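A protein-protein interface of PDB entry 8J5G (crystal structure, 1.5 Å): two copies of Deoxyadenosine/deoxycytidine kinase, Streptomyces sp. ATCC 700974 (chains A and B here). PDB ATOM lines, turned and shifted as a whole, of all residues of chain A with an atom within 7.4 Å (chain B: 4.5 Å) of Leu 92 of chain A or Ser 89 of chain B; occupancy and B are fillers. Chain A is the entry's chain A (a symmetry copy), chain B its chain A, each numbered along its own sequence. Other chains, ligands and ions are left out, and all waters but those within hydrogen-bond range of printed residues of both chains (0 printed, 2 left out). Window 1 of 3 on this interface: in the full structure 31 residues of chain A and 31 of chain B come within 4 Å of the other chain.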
ATOM      1  N   PHE A  67     -27.663  34.098  18.476  1.00  0.00           N
ATOM      2  CA  PHE A  67     -26.974  32.862  18.827  1.00  0.00           C
ATOM      3  C   PHE A  67     -25.977  32.397  17.773  1.00  0.00           C
ATOM      4  O   PHE A  67     -25.387  31.323  17.932  1.00  0.00           O
ATOM      5  CB  PHE A  67     -27.998  31.755  19.078  1.00  0.00           C
ATOM      6  CG  PHE A  67     -28.983  32.089  20.146  1.00  0.00           C
ATOM      7  CD1 PHE A  67     -28.550  32.491  21.402  1.00  0.00           C
ATOM      8  CD2 PHE A  67     -30.346  32.029  19.896  1.00  0.00           C
ATOM      9  CE1 PHE A  67     -29.455  32.817  22.394  1.00  0.00           C
ATOM     10  CE2 PHE A  67     -31.262  32.353  20.882  1.00  0.00           C
ATOM     11  CZ  PHE A  67     -30.821  32.745  22.136  1.00  0.00           C
ATOM     12  N   PRO A  85     -19.485  20.901  18.047  1.00  0.00           N
ATOM     13  CA  PRO A  85     -19.362  22.012  19.006  1.00  0.00           C
ATOM     14  C   PRO A  85     -20.232  23.211  18.662  1.00  0.00           C
ATOM     15  O   PRO A  85     -20.711  23.887  19.584  1.00  0.00           O
ATOM     16  CB  PRO A  85     -17.866  22.352  18.973  1.00  0.00           C
ATOM     17  CG  PRO A  85     -17.382  21.830  17.651  1.00  0.00           C
ATOM     18  CD  PRO A  85     -18.191  20.599  17.398  1.00  0.00           C
ATOM     19  N   ILE A  86     -20.491  23.494  17.381  1.00  0.00           N
ATOM     20  CA  ILE A  86     -21.383  24.614  17.072  1.00  0.00           C
ATOM     21  C   ILE A  86     -22.829  24.283  17.435  1.00  0.00           C
ATOM     22  O   ILE A  86     -23.578  25.160  17.894  1.00  0.00           O
ATOM     23  CB  ILE A  86     -21.240  25.051  15.603  1.00  0.00           C
ATOM     24  CG1 ILE A  86     -19.831  25.579  15.345  1.00  0.00           C
ATOM     25  CG2 ILE A  86     -22.300  26.123  15.269  1.00  0.00           C
ATOM     26  CD1 ILE A  86     -19.512  26.883  16.040  1.00  0.00           C
ATOM     27  N   GLN A  87     -23.253  23.022  17.275  1.00  0.00           N
ATOM     28  CA  GLN A  87     -24.570  22.645  17.795  1.00  0.00           C
ATOM     29  C   GLN A  87     -24.627  22.749  19.318  1.00  0.00           C
ATOM     30  O   GLN A  87     -25.657  23.140  19.879  1.00  0.00           O
ATOM     31  CB  GLN A  87     -24.955  21.234  17.360  1.00  0.00           C
ATOM     32  CG  GLN A  87     -25.364  21.140  15.893  1.00  0.00           C
ATOM     33  CD  GLN A  87     -26.538  22.040  15.552  1.00  0.00           C
ATOM     34  OE1 GLN A  87     -26.573  22.671  14.488  1.00  0.00           O
ATOM     35  NE2 GLN A  87     -27.520  22.078  16.426  1.00  0.00           N
ATOM     36  N   LEU A  88     -23.547  22.371  20.011  1.00  0.00           N
ATOM     37  CA  LEU A  88     -23.517  22.599  21.456  1.00  0.00           C
ATOM     38  C   LEU A  88     -23.679  24.079  21.776  1.00  0.00           C
ATOM     39  O   LEU A  88     -24.360  24.441  22.750  1.00  0.00           O
ATOM     40  CB  LEU A  88     -22.215  22.061  22.059  1.00  0.00           C
ATOM     41  CG  LEU A  88     -22.067  20.541  22.166  1.00  0.00           C
ATOM     42  CD1 LEU A  88     -20.608  20.175  22.438  1.00  0.00           C
ATOM     43  CD2 LEU A  88     -22.989  19.970  23.245  1.00  0.00           C
ATOM     44  N   SER A  89     -23.074  24.951  20.957  1.00  0.00           N
ATOM     45  CA  SER A  89     -23.158  26.391  21.204  1.00  0.00           C
ATOM     46  C   SER A  89     -24.584  26.917  21.046  1.00  0.00           C
ATOM     47  O   SER A  89     -25.047  27.726  21.872  1.00  0.00           O
ATOM     48  CB  SER A  89     -22.192  27.132  20.275  1.00  0.00           C
ATOM     49  OG  SER A  89     -22.299  28.541  20.463  1.00  0.00           O
ATOM     50  N   PHE A  90     -25.293  26.490  19.995  1.00  0.00           N
ATOM     51  CA  PHE A  90     -26.677  26.926  19.821  1.00  0.00           C
ATOM     52  C   PHE A  90     -27.498  26.544  21.048  1.00  0.00           C
ATOM     53  O   PHE A  90     -28.216  27.381  21.622  1.00  0.00           O
ATOM     54  CB  PHE A  90     -27.296  26.301  18.564  1.00  0.00           C
ATOM     55  CG  PHE A  90     -27.168  27.147  17.305  1.00  0.00           C
ATOM     56  CD1 PHE A  90     -27.910  28.309  17.143  1.00  0.00           C
ATOM     57  CD2 PHE A  90     -26.349  26.736  16.262  1.00  0.00           C
ATOM     58  CE1 PHE A  90     -27.804  29.075  15.980  1.00  0.00           C
ATOM     59  CE2 PHE A  90     -26.251  27.485  15.092  1.00  0.00           C
ATOM     60  CZ  PHE A  90     -26.968  28.650  14.948  1.00  0.00           C
ATOM     61  N   MET A  91     -27.372  25.293  21.509  1.00  0.00           N
ATOM     62  CA  MET A  91     -28.267  24.944  22.602  1.00  0.00           C
ATOM     63  C   MET A  91     -27.816  25.569  23.916  1.00  0.00           C
ATOM     64  O   MET A  91     -28.673  25.986  24.711  1.00  0.00           O
ATOM     65  CB  MET A  91     -28.486  23.422  22.721  1.00  0.00           C
ATOM     66  CG  MET A  91     -28.584  22.798  24.147  1.00  0.00           C
ATOM     67  SD  MET A  91     -28.108  21.057  24.340  1.00  0.00           S
ATOM     68  CE  MET A  91     -26.339  21.166  24.442  1.00  0.00           C
ATOM     69  N   LEU A  92     -26.506  25.742  24.114  1.00  0.00           N
ATOM     70  CA  LEU A  92     -26.013  26.333  25.360  1.00  0.00           C
ATOM     71  C   LEU A  92     -26.365  27.818  25.473  1.00  0.00           C
ATOM     72  O   LEU A  92     -26.833  28.278  26.525  1.00  0.00           O
ATOM     73  CB  LEU A  92     -24.503  26.135  25.474  1.00  0.00           C
ATOM     74  CG  LEU A  92     -23.913  26.713  26.761  1.00  0.00           C
ATOM     75  CD1 LEU A  92     -24.530  26.080  28.009  1.00  0.00           C
ATOM     76  CD2 LEU A  92     -22.410  26.499  26.743  1.00  0.00           C
ATOM     77  N   GLU A  93     -26.150  28.585  24.397  1.00  0.00           N
ATOM     78  CA  GLU A  93     -26.413  30.021  24.450  1.00  0.00           C
ATOM     79  C   GLU A  93     -27.905  30.303  24.544  1.00  0.00           C
ATOM     80  O   GLU A  93     -28.328  31.204  25.289  1.00  0.00           O
ATOM     81  CB  GLU A  93     -25.806  30.735  23.238  1.00  0.00           C
ATOM     82  CG  GLU A  93     -24.277  30.618  23.149  1.00  0.00           C
ATOM     83  CD  GLU A  93     -23.541  31.357  24.271  1.00  0.00           C
ATOM     84  OE1 GLU A  93     -24.147  32.181  24.984  1.00  0.00           O
ATOM     85  OE2 GLU A  93     -22.327  31.107  24.444  1.00  0.00           O
ATOM     86  N   ARG A  94     -28.721  29.521  23.831  1.00  0.00           N
ATOM     87  CA  ARG A  94     -30.170  29.648  23.991  1.00  0.00           C
ATOM     88  C   ARG A  94     -30.581  29.322  25.419  1.00  0.00           C
ATOM     89  O   ARG A  94     -31.390  30.042  26.026  1.00  0.00           O
ATOM     90  CB  ARG A  94     -30.895  28.730  23.006  1.00  0.00           C
ATOM     91  CG  ARG A  94     -32.388  29.051  22.865  1.00  0.00           C
ATOM     92  CD  ARG A  94     -33.170  27.952  22.132  1.00  0.00           C
ATOM     93  NE  ARG A  94     -32.493  27.505  20.917  1.00  0.00           N
ATOM     94  CZ  ARG A  94     -32.339  28.235  19.820  1.00  0.00           C
ATOM     95  NH1 ARG A  94     -32.897  29.430  19.692  1.00  0.00           N
ATOM     96  NH2 ARG A  94     -31.578  27.763  18.832  1.00  0.00           N
ATOM     97  N   HIS A  95     -30.023  28.245  25.973  1.00  0.00           N
ATOM     98  CA  HIS A  95     -30.339  27.857  27.346  1.00  0.00           C
ATOM     99  C   HIS A  95     -30.032  28.974  28.336  1.00  0.00           C
ATOM    100  O   HIS A  95     -30.859  29.297  29.203  1.00  0.00           O
ATOM    101  CB  HIS A  95     -29.545  26.608  27.739  1.00  0.00           C
ATOM    102  CG  HIS A  95     -29.721  26.244  29.176  1.00  0.00           C
ATOM    103  ND1 HIS A  95     -30.807  25.521  29.623  1.00  0.00           N
ATOM    104  CD2 HIS A  95     -28.999  26.566  30.277  1.00  0.00           C
ATOM    105  CE1 HIS A  95     -30.727  25.390  30.937  1.00  0.00           C
ATOM    106  NE2 HIS A  95     -29.645  26.018  31.360  1.00  0.00           N
ATOM    107  N   LEU A  96     -28.823  29.544  28.253  1.00  0.00           N
ATOM    108  CA  LEU A  96     -28.410  30.582  29.199  1.00  0.00           C
ATOM    109  C   LEU A  96     -29.307  31.808  29.094  1.00  0.00           C
ATOM    110  O   LEU A  96     -29.733  32.370  30.114  1.00  0.00           O
ATOM    111  CB  LEU A  96     -26.953  30.967  28.939  1.00  0.00           C
ATOM    112  CG  LEU A  96     -25.924  30.014  29.522  1.00  0.00           C
ATOM    113  CD1 LEU A  96     -24.582  30.285  28.856  1.00  0.00           C
ATOM    114  CD2 LEU A  96     -25.849  30.222  31.035  1.00  0.00           C
ATOM    115  N   LEU A  97     -29.627  32.222  27.868  1.00  0.00           N
ATOM    116  CA  LEU A  97     -30.484  33.393  27.700  1.00  0.00           C
ATOM    117  C   LEU A  97     -31.878  33.155  28.282  1.00  0.00           C
ATOM    118  O   LEU A  97     -32.455  34.052  28.922  1.00  0.00           O
ATOM    119  CB  LEU A  97     -30.552  33.771  26.216  1.00  0.00           C
ATOM    120  CG  LEU A  97     -31.186  35.133  25.956  1.00  0.00           C
ATOM    121  CD1 LEU A  97     -30.114  36.181  25.771  1.00  0.00           C
ATOM    122  CD2 LEU A  97     -32.071  35.077  24.739  1.00  0.00           C
ATOM    123  N   LEU A  98     -32.435  31.955  28.072  1.00  0.00           N
ATOM    124  CA  LEU A  98     -33.728  31.614  28.662  1.00  0.00           C
ATOM    125  C   LEU A  98     -33.633  31.491  30.179  1.00  0.00           C
ATOM    126  O   LEU A  98     -34.511  31.983  30.907  1.00  0.00           O
ATOM    127  CB  LEU A  98     -34.249  30.304  28.067  1.00  0.00           C
ATOM    128  CG  LEU A  98     -34.682  30.302  26.597  1.00  0.00           C
ATOM    129  CD1 LEU A  98     -34.798  28.871  26.089  1.00  0.00           C
ATOM    130  CD2 LEU A  98     -36.002  31.036  26.426  1.00  0.00           C
ATOM    131  N   ASP A 118     -33.601  22.390  18.799  1.00  0.00           N
ATOM    132  CA  ASP A 118     -32.180  22.242  18.465  1.00  0.00           C
ATOM    133  C   ASP A 118     -31.799  20.793  18.160  1.00  0.00           C
ATOM    134  O   ASP A 118     -30.918  20.542  17.315  1.00  0.00           O
ATOM    135  CB  ASP A 118     -31.303  22.780  19.603  1.00  0.00           C
ATOM    136  CG  ASP A 118     -31.302  24.293  19.683  1.00  0.00           C
ATOM    137  OD1 ASP A 118     -31.149  24.958  18.641  1.00  0.00           O
ATOM    138  OD2 ASP A 118     -31.451  24.822  20.804  1.00  0.00           O
ATOM    139  N   TYR A 139     -24.303  14.774  23.490  1.00  0.00           N
ATOM    140  CA  TYR A 139     -25.181  15.929  23.310  1.00  0.00           C
ATOM    141  C   TYR A 139     -26.518  15.729  24.016  1.00  0.00           C
ATOM    142  O   TYR A 139     -27.016  16.627  24.705  1.00  0.00           O
ATOM    143  CB  TYR A 139     -25.407  16.169  21.816  1.00  0.00           C
ATOM    144  CG  TYR A 139     -26.392  17.270  21.503  1.00  0.00           C
ATOM    145  CD1 TYR A 139     -27.762  17.007  21.418  1.00  0.00           C
ATOM    146  CD2 TYR A 139     -25.962  18.577  21.316  1.00  0.00           C
ATOM    147  CE1 TYR A 139     -28.667  18.018  21.144  1.00  0.00           C
ATOM    148  CE2 TYR A 139     -26.860  19.600  21.042  1.00  0.00           C
ATOM    149  CZ  TYR A 139     -28.214  19.311  20.952  1.00  0.00           C
ATOM    150  OH  TYR A 139     -29.118  20.300  20.659  1.00  0.00           O
ATOM    151  N   VAL A 142     -26.423  16.050  27.896  1.00  0.00           N
ATOM    152  CA  VAL A 142     -26.401  17.440  28.341  1.00  0.00           C
ATOM    153  C   VAL A 142     -27.728  18.129  28.043  1.00  0.00           C
ATOM    154  O   VAL A 142     -28.273  18.841  28.895  1.00  0.00           O
ATOM    155  CB  VAL A 142     -25.224  18.185  27.695  1.00  0.00           C
ATOM    156  CG1 VAL A 142     -25.386  19.697  27.874  1.00  0.00           C
ATOM    157  CG2 VAL A 142     -23.925  17.717  28.324  1.00  0.00           C
ATOM    158  N   LEU A 146     -30.138  20.246  30.628  1.00  0.00           N
ATOM    159  CA  LEU A 146     -30.412  21.663  30.414  1.00  0.00           C
ATOM    160  C   LEU A 146     -31.908  21.903  30.263  1.00  0.00           C
ATOM    161  O   LEU A 146     -32.479  22.793  30.911  1.00  0.00           O
ATOM    162  CB  LEU A 146     -29.664  22.157  29.176  1.00  0.00           C
ATOM    163  CG  LEU A 146     -28.141  22.226  29.278  1.00  0.00           C
ATOM    164  CD1 LEU A 146     -27.591  22.684  27.915  1.00  0.00           C
ATOM    165  CD2 LEU A 146     -27.689  23.180  30.377  1.00  0.00           C
ATOM    166  N   HIS B  69     -17.905  34.553  29.873  1.00  0.00           N
ATOM    167  CA  HIS B  69     -19.249  34.783  29.380  1.00  0.00           C
ATOM    168  C   HIS B  69     -19.820  36.080  29.945  1.00  0.00           C
ATOM    169  O   HIS B  69     -19.489  36.493  31.061  1.00  0.00           O
ATOM    170  CB  HIS B  69     -20.152  33.611  29.767  1.00  0.00           C
ATOM    171  CG  HIS B  69     -21.358  33.482  28.902  1.00  0.00           C
ATOM    172  ND1 HIS B  69     -22.484  34.256  29.081  1.00  0.00           N
ATOM    173  CD2 HIS B  69     -21.606  32.695  27.833  1.00  0.00           C
ATOM    174  CE1 HIS B  69     -23.378  33.944  28.162  1.00  0.00           C
ATOM    175  NE2 HIS B  69     -22.860  33.013  27.375  1.00  0.00           N
ATOM    176  N   PRO B  85     -24.153  25.478  33.250  1.00  0.00           N
ATOM    177  CA  PRO B  85     -24.027  25.996  31.877  1.00  0.00           C
ATOM    178  C   PRO B  85     -22.832  26.917  31.683  1.00  0.00           C
ATOM    179  O   PRO B  85     -22.249  26.918  30.588  1.00  0.00           O
ATOM    180  CB  PRO B  85     -25.360  26.718  31.640  1.00  0.00           C
ATOM    181  CG  PRO B  85     -25.875  27.034  33.015  1.00  0.00           C
ATOM    182  CD  PRO B  85     -25.429  25.893  33.870  1.00  0.00           C
ATOM    183  N   ILE B  86     -22.413  27.679  32.699  1.00  0.00           N
ATOM    184  CA  ILE B  86     -21.221  28.511  32.511  1.00  0.00           C
ATOM    185  C   ILE B  86     -19.956  27.657  32.449  1.00  0.00           C
ATOM    186  O   ILE B  86     -19.026  27.967  31.689  1.00  0.00           O
ATOM    187  CB  ILE B  86     -21.130  29.604  33.591  1.00  0.00           C
ATOM    188  CG1 ILE B  86     -22.310  30.564  33.472  1.00  0.00           C
ATOM    189  CG2 ILE B  86     -19.790  30.359  33.462  1.00  0.00           C
ATOM    190  CD1 ILE B  86     -22.298  31.421  32.228  1.00  0.00           C
ATOM    191  N   GLN B  87     -19.895  26.555  33.210  1.00  0.00           N
ATOM    192  CA  GLN B  87     -18.778  25.625  33.021  1.00  0.00           C
ATOM    193  C   GLN B  87     -18.804  24.985  31.635  1.00  0.00           C
ATOM    194  O   GLN B  87     -17.748  24.760  31.032  1.00  0.00           O
ATOM    195  CB  GLN B  87     -18.776  24.537  34.091  1.00  0.00           C
ATOM    196  CG  GLN B  87     -18.306  25.027  35.457  1.00  0.00           C
ATOM    197  CD  GLN B  87     -16.905  25.611  35.422  1.00  0.00           C
ATOM    198  OE1 GLN B  87     -16.617  26.626  36.067  1.00  0.00           O
ATOM    199  NE2 GLN B  87     -16.018  24.957  34.704  1.00  0.00           N
ATOM    200  N   LEU B  88     -19.993  24.649  31.123  1.00  0.00           N
ATOM    201  CA  LEU B  88     -20.061  24.174  29.741  1.00  0.00           C
ATOM    202  C   LEU B  88     -19.512  25.219  28.779  1.00  0.00           C
ATOM    203  O   LEU B  88     -18.828  24.876  27.800  1.00  0.00           O
ATOM    204  CB  LEU B  88     -21.501  23.808  29.368  1.00  0.00           C
ATOM    205  CG  LEU B  88     -22.079  22.525  29.973  1.00  0.00           C
ATOM    206  CD1 LEU B  88     -23.598  22.503  29.799  1.00  0.00           C
ATOM    207  CD2 LEU B  88     -21.435  21.284  29.354  1.00  0.00           C
ATOM    208  N   SER B  89     -19.786  26.503  29.051  1.00  0.00           N
ATOM    209  CA  SER B  89     -19.318  27.570  28.167  1.00  0.00           C
ATOM    210  C   SER B  89     -17.793  27.684  28.163  1.00  0.00           C
ATOM    211  O   SER B  89     -17.182  27.846  27.090  1.00  0.00           O
ATOM    212  CB  SER B  89     -19.967  28.898  28.570  1.00  0.00           C
ATOM    213  OG  SER B  89     -19.481  29.961  27.754  1.00  0.00           O
ATOM    214  N   PHE B  90     -17.161  27.617  29.339  1.00  0.00           N
ATOM    215  CA  PHE B  90     -15.701  27.673  29.387  1.00  0.00           C
ATOM    216  C   PHE B  90     -15.111  26.550  28.544  1.00  0.00           C
ATOM    217  O   PHE B  90     -14.229  26.781  27.698  1.00  0.00           O
ATOM    218  CB  PHE B  90     -15.195  27.562  30.832  1.00  0.00           C
ATOM    219  CG  PHE B  90     -14.988  28.896  31.537  1.00  0.00           C
ATOM    220  CD1 PHE B  90     -13.939  29.736  31.190  1.00  0.00           C
ATOM    221  CD2 PHE B  90     -15.814  29.269  32.589  1.00  0.00           C
ATOM    222  CE1 PHE B  90     -13.743  30.951  31.850  1.00  0.00           C
ATOM    223  CE2 PHE B  90     -15.613  30.470  33.265  1.00  0.00           C
ATOM    224  CZ  PHE B  90     -14.588  31.312  32.899  1.00  0.00           C
ATOM    225  N   MET B  91     -15.617  25.321  28.713  1.00  0.00           N
ATOM    226  CA  MET B  91     -14.937  24.266  27.976  1.00  0.00           C
ATOM    227  C   MET B  91     -15.286  24.304  26.494  1.00  0.00           C
ATOM    228  O   MET B  91     -14.406  24.040  25.659  1.00  0.00           O
ATOM    229  CB  MET B  91     -15.165  22.873  28.597  1.00  0.00           C
ATOM    230  CG  MET B  91     -15.349  21.656  27.638  1.00  0.00           C
ATOM    231  SD  MET B  91     -16.309  20.241  28.247  1.00  0.00           S
ATOM    232  CE  MET B  91     -17.978  20.784  27.980  1.00  0.00           C
ATOM    233  N   LEU B  92     -16.506  24.725  26.144  1.00  0.00           N
ATOM    234  CA  LEU B  92     -16.899  24.777  24.735  1.00  0.00           C
ATOM    235  C   LEU B  92     -16.152  25.870  23.967  1.00  0.00           C
ATOM    236  O   LEU B  92     -15.651  25.633  22.859  1.00  0.00           O
ATOM    237  CB  LEU B  92     -18.408  24.984  24.618  1.00  0.00           C
ATOM    238  CG  LEU B  92     -18.903  25.033  23.172  1.00  0.00           C
ATOM    239  CD1 LEU B  92     -18.580  23.747  22.412  1.00  0.00           C
ATOM    240  CD2 LEU B  92     -20.400  25.286  23.181  1.00  0.00           C
ATOM    241  N   GLU B  93     -16.066  27.076  24.542  1.00  0.00           N
ATOM    242  CA  GLU B  93     -15.413  28.181  23.843  1.00  0.00           C
ATOM    243  C   GLU B  93     -13.912  27.953  23.736  1.00  0.00           C
ATOM    244  O   GLU B  93     -13.307  28.241  22.689  1.00  0.00           O
ATOM    245  CB  GLU B  93     -15.706  29.517  24.535  1.00  0.00           C
ATOM    246  CG  GLU B  93     -17.195  29.891  24.558  1.00  0.00           C
ATOM    247  CD  GLU B  93     -17.772  30.193  23.172  1.00  0.00           C
ATOM    248  OE1 GLU B  93     -17.011  30.381  22.203  1.00  0.00           O
ATOM    249  OE2 GLU B  93     -19.016  30.245  23.050  1.00  0.00           O
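Pro 85 of chain A touches Leu 92 of chain B, and with the chains exchanged Leu 92 of chain A touches Pro 85 of chain B.
Leu 88 of chain A touches Leu 92 of chain B, and with the chains exchanged Leu 92 of chain A touches Leu 88 of chain B.
Ser 89 of chain A touches Leu 92 of chain B, and with the chains exchanged Leu 92 of chain A touches Ser 89 of chain B.
Glu 93 of chain B touches its own counterpart, Glu 93 of chain A.
Positions printed for both chains: 85, 86, 87, 88, 89, 90, 91, 92 and 93.
Ser 89 of chain B touches just one residue of chain A: Leu 92 (3.5 Å).
Of the printed residues of chain A, Ile 86 of chain B touches Leu 96 (3.9 Å).
Of the printed residues of chain A, Pro 85 of chain B touches Leu 92, His 95 and Leu 96.
Printed residues of chain A within 4 Å of Leu 92 of chain B: Pro 85, Leu 88 and Ser 89.
Of the printed residues of chain B, Pro 85 of chain A touches Leu 92 (3.5 Å).
Printed residues of chain B within 4 Å of Val 142 of chain A: Leu 88 (3.8 Å).
The nearest residue of chain B that does not touch Leu 92 of chain A is Leu 92 of chain B (4.3 Å).
The nearest printed residue of chain A that does not touch Pro 85 of chain B is Leu 146 of chain A (4.4 Å).
The side-chain carboxylate of Glu 93 of chain A lies within hydrogen-bond range of a ring nitrogen (NE2) of His 69 of chain B.
Among the printed residues, merely in contact across the chains: Ser 89 of chain A with Leu 92 of chain B (3.5 Å), Leu 92 of chain A with Ser 89 of chain B (3.5 Å), Leu 92 of chain A with Pro 85 of chain B (3.5 Å), Pro 85 of chain A with Leu 92 of chain B (3.5 Å), Leu 96 of chain A with His 69 of chain B (3.5 Å), Leu 96 of chain A with Pro 85 of chain B (3.6 Å), Glu 93 of chain A with Glu 93 of chain B (3.7 Å), Leu 92 of chain A with Leu 88 of chain B (3.8 Å), Leu 88 of chain A with Leu 92 of chain B (3.8 Å), Val 142 of chain A with Leu 88 of chain B (3.8 Å), His 95 of chain A with Pro 85 of chain B (3.9 Å) and Leu 96 of chain A with Ile 86 of chain B (3.9 Å).
Of the 10 printed residues of chain B, 7 touch a printed residue of chain A.
Hydrophobic or aromatic side chains of chain A within 4 Å of the printed part of chain B: Pro 85, Leu 88, Leu 92, His 95, Leu 96 and Val 142.
Among the printed residues, 13 pairs touch across the chains.
Among the printed residues, no Asp or Glu carboxylate lies within 4 Å of a Lys or Arg side-chain nitrogen of the other chain.
A ring nitrogen (ND1) of His 95 of chain A lies close to the backbone carbonyl oxygen (O) of Leu 146 of chain A (3.4 Å).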
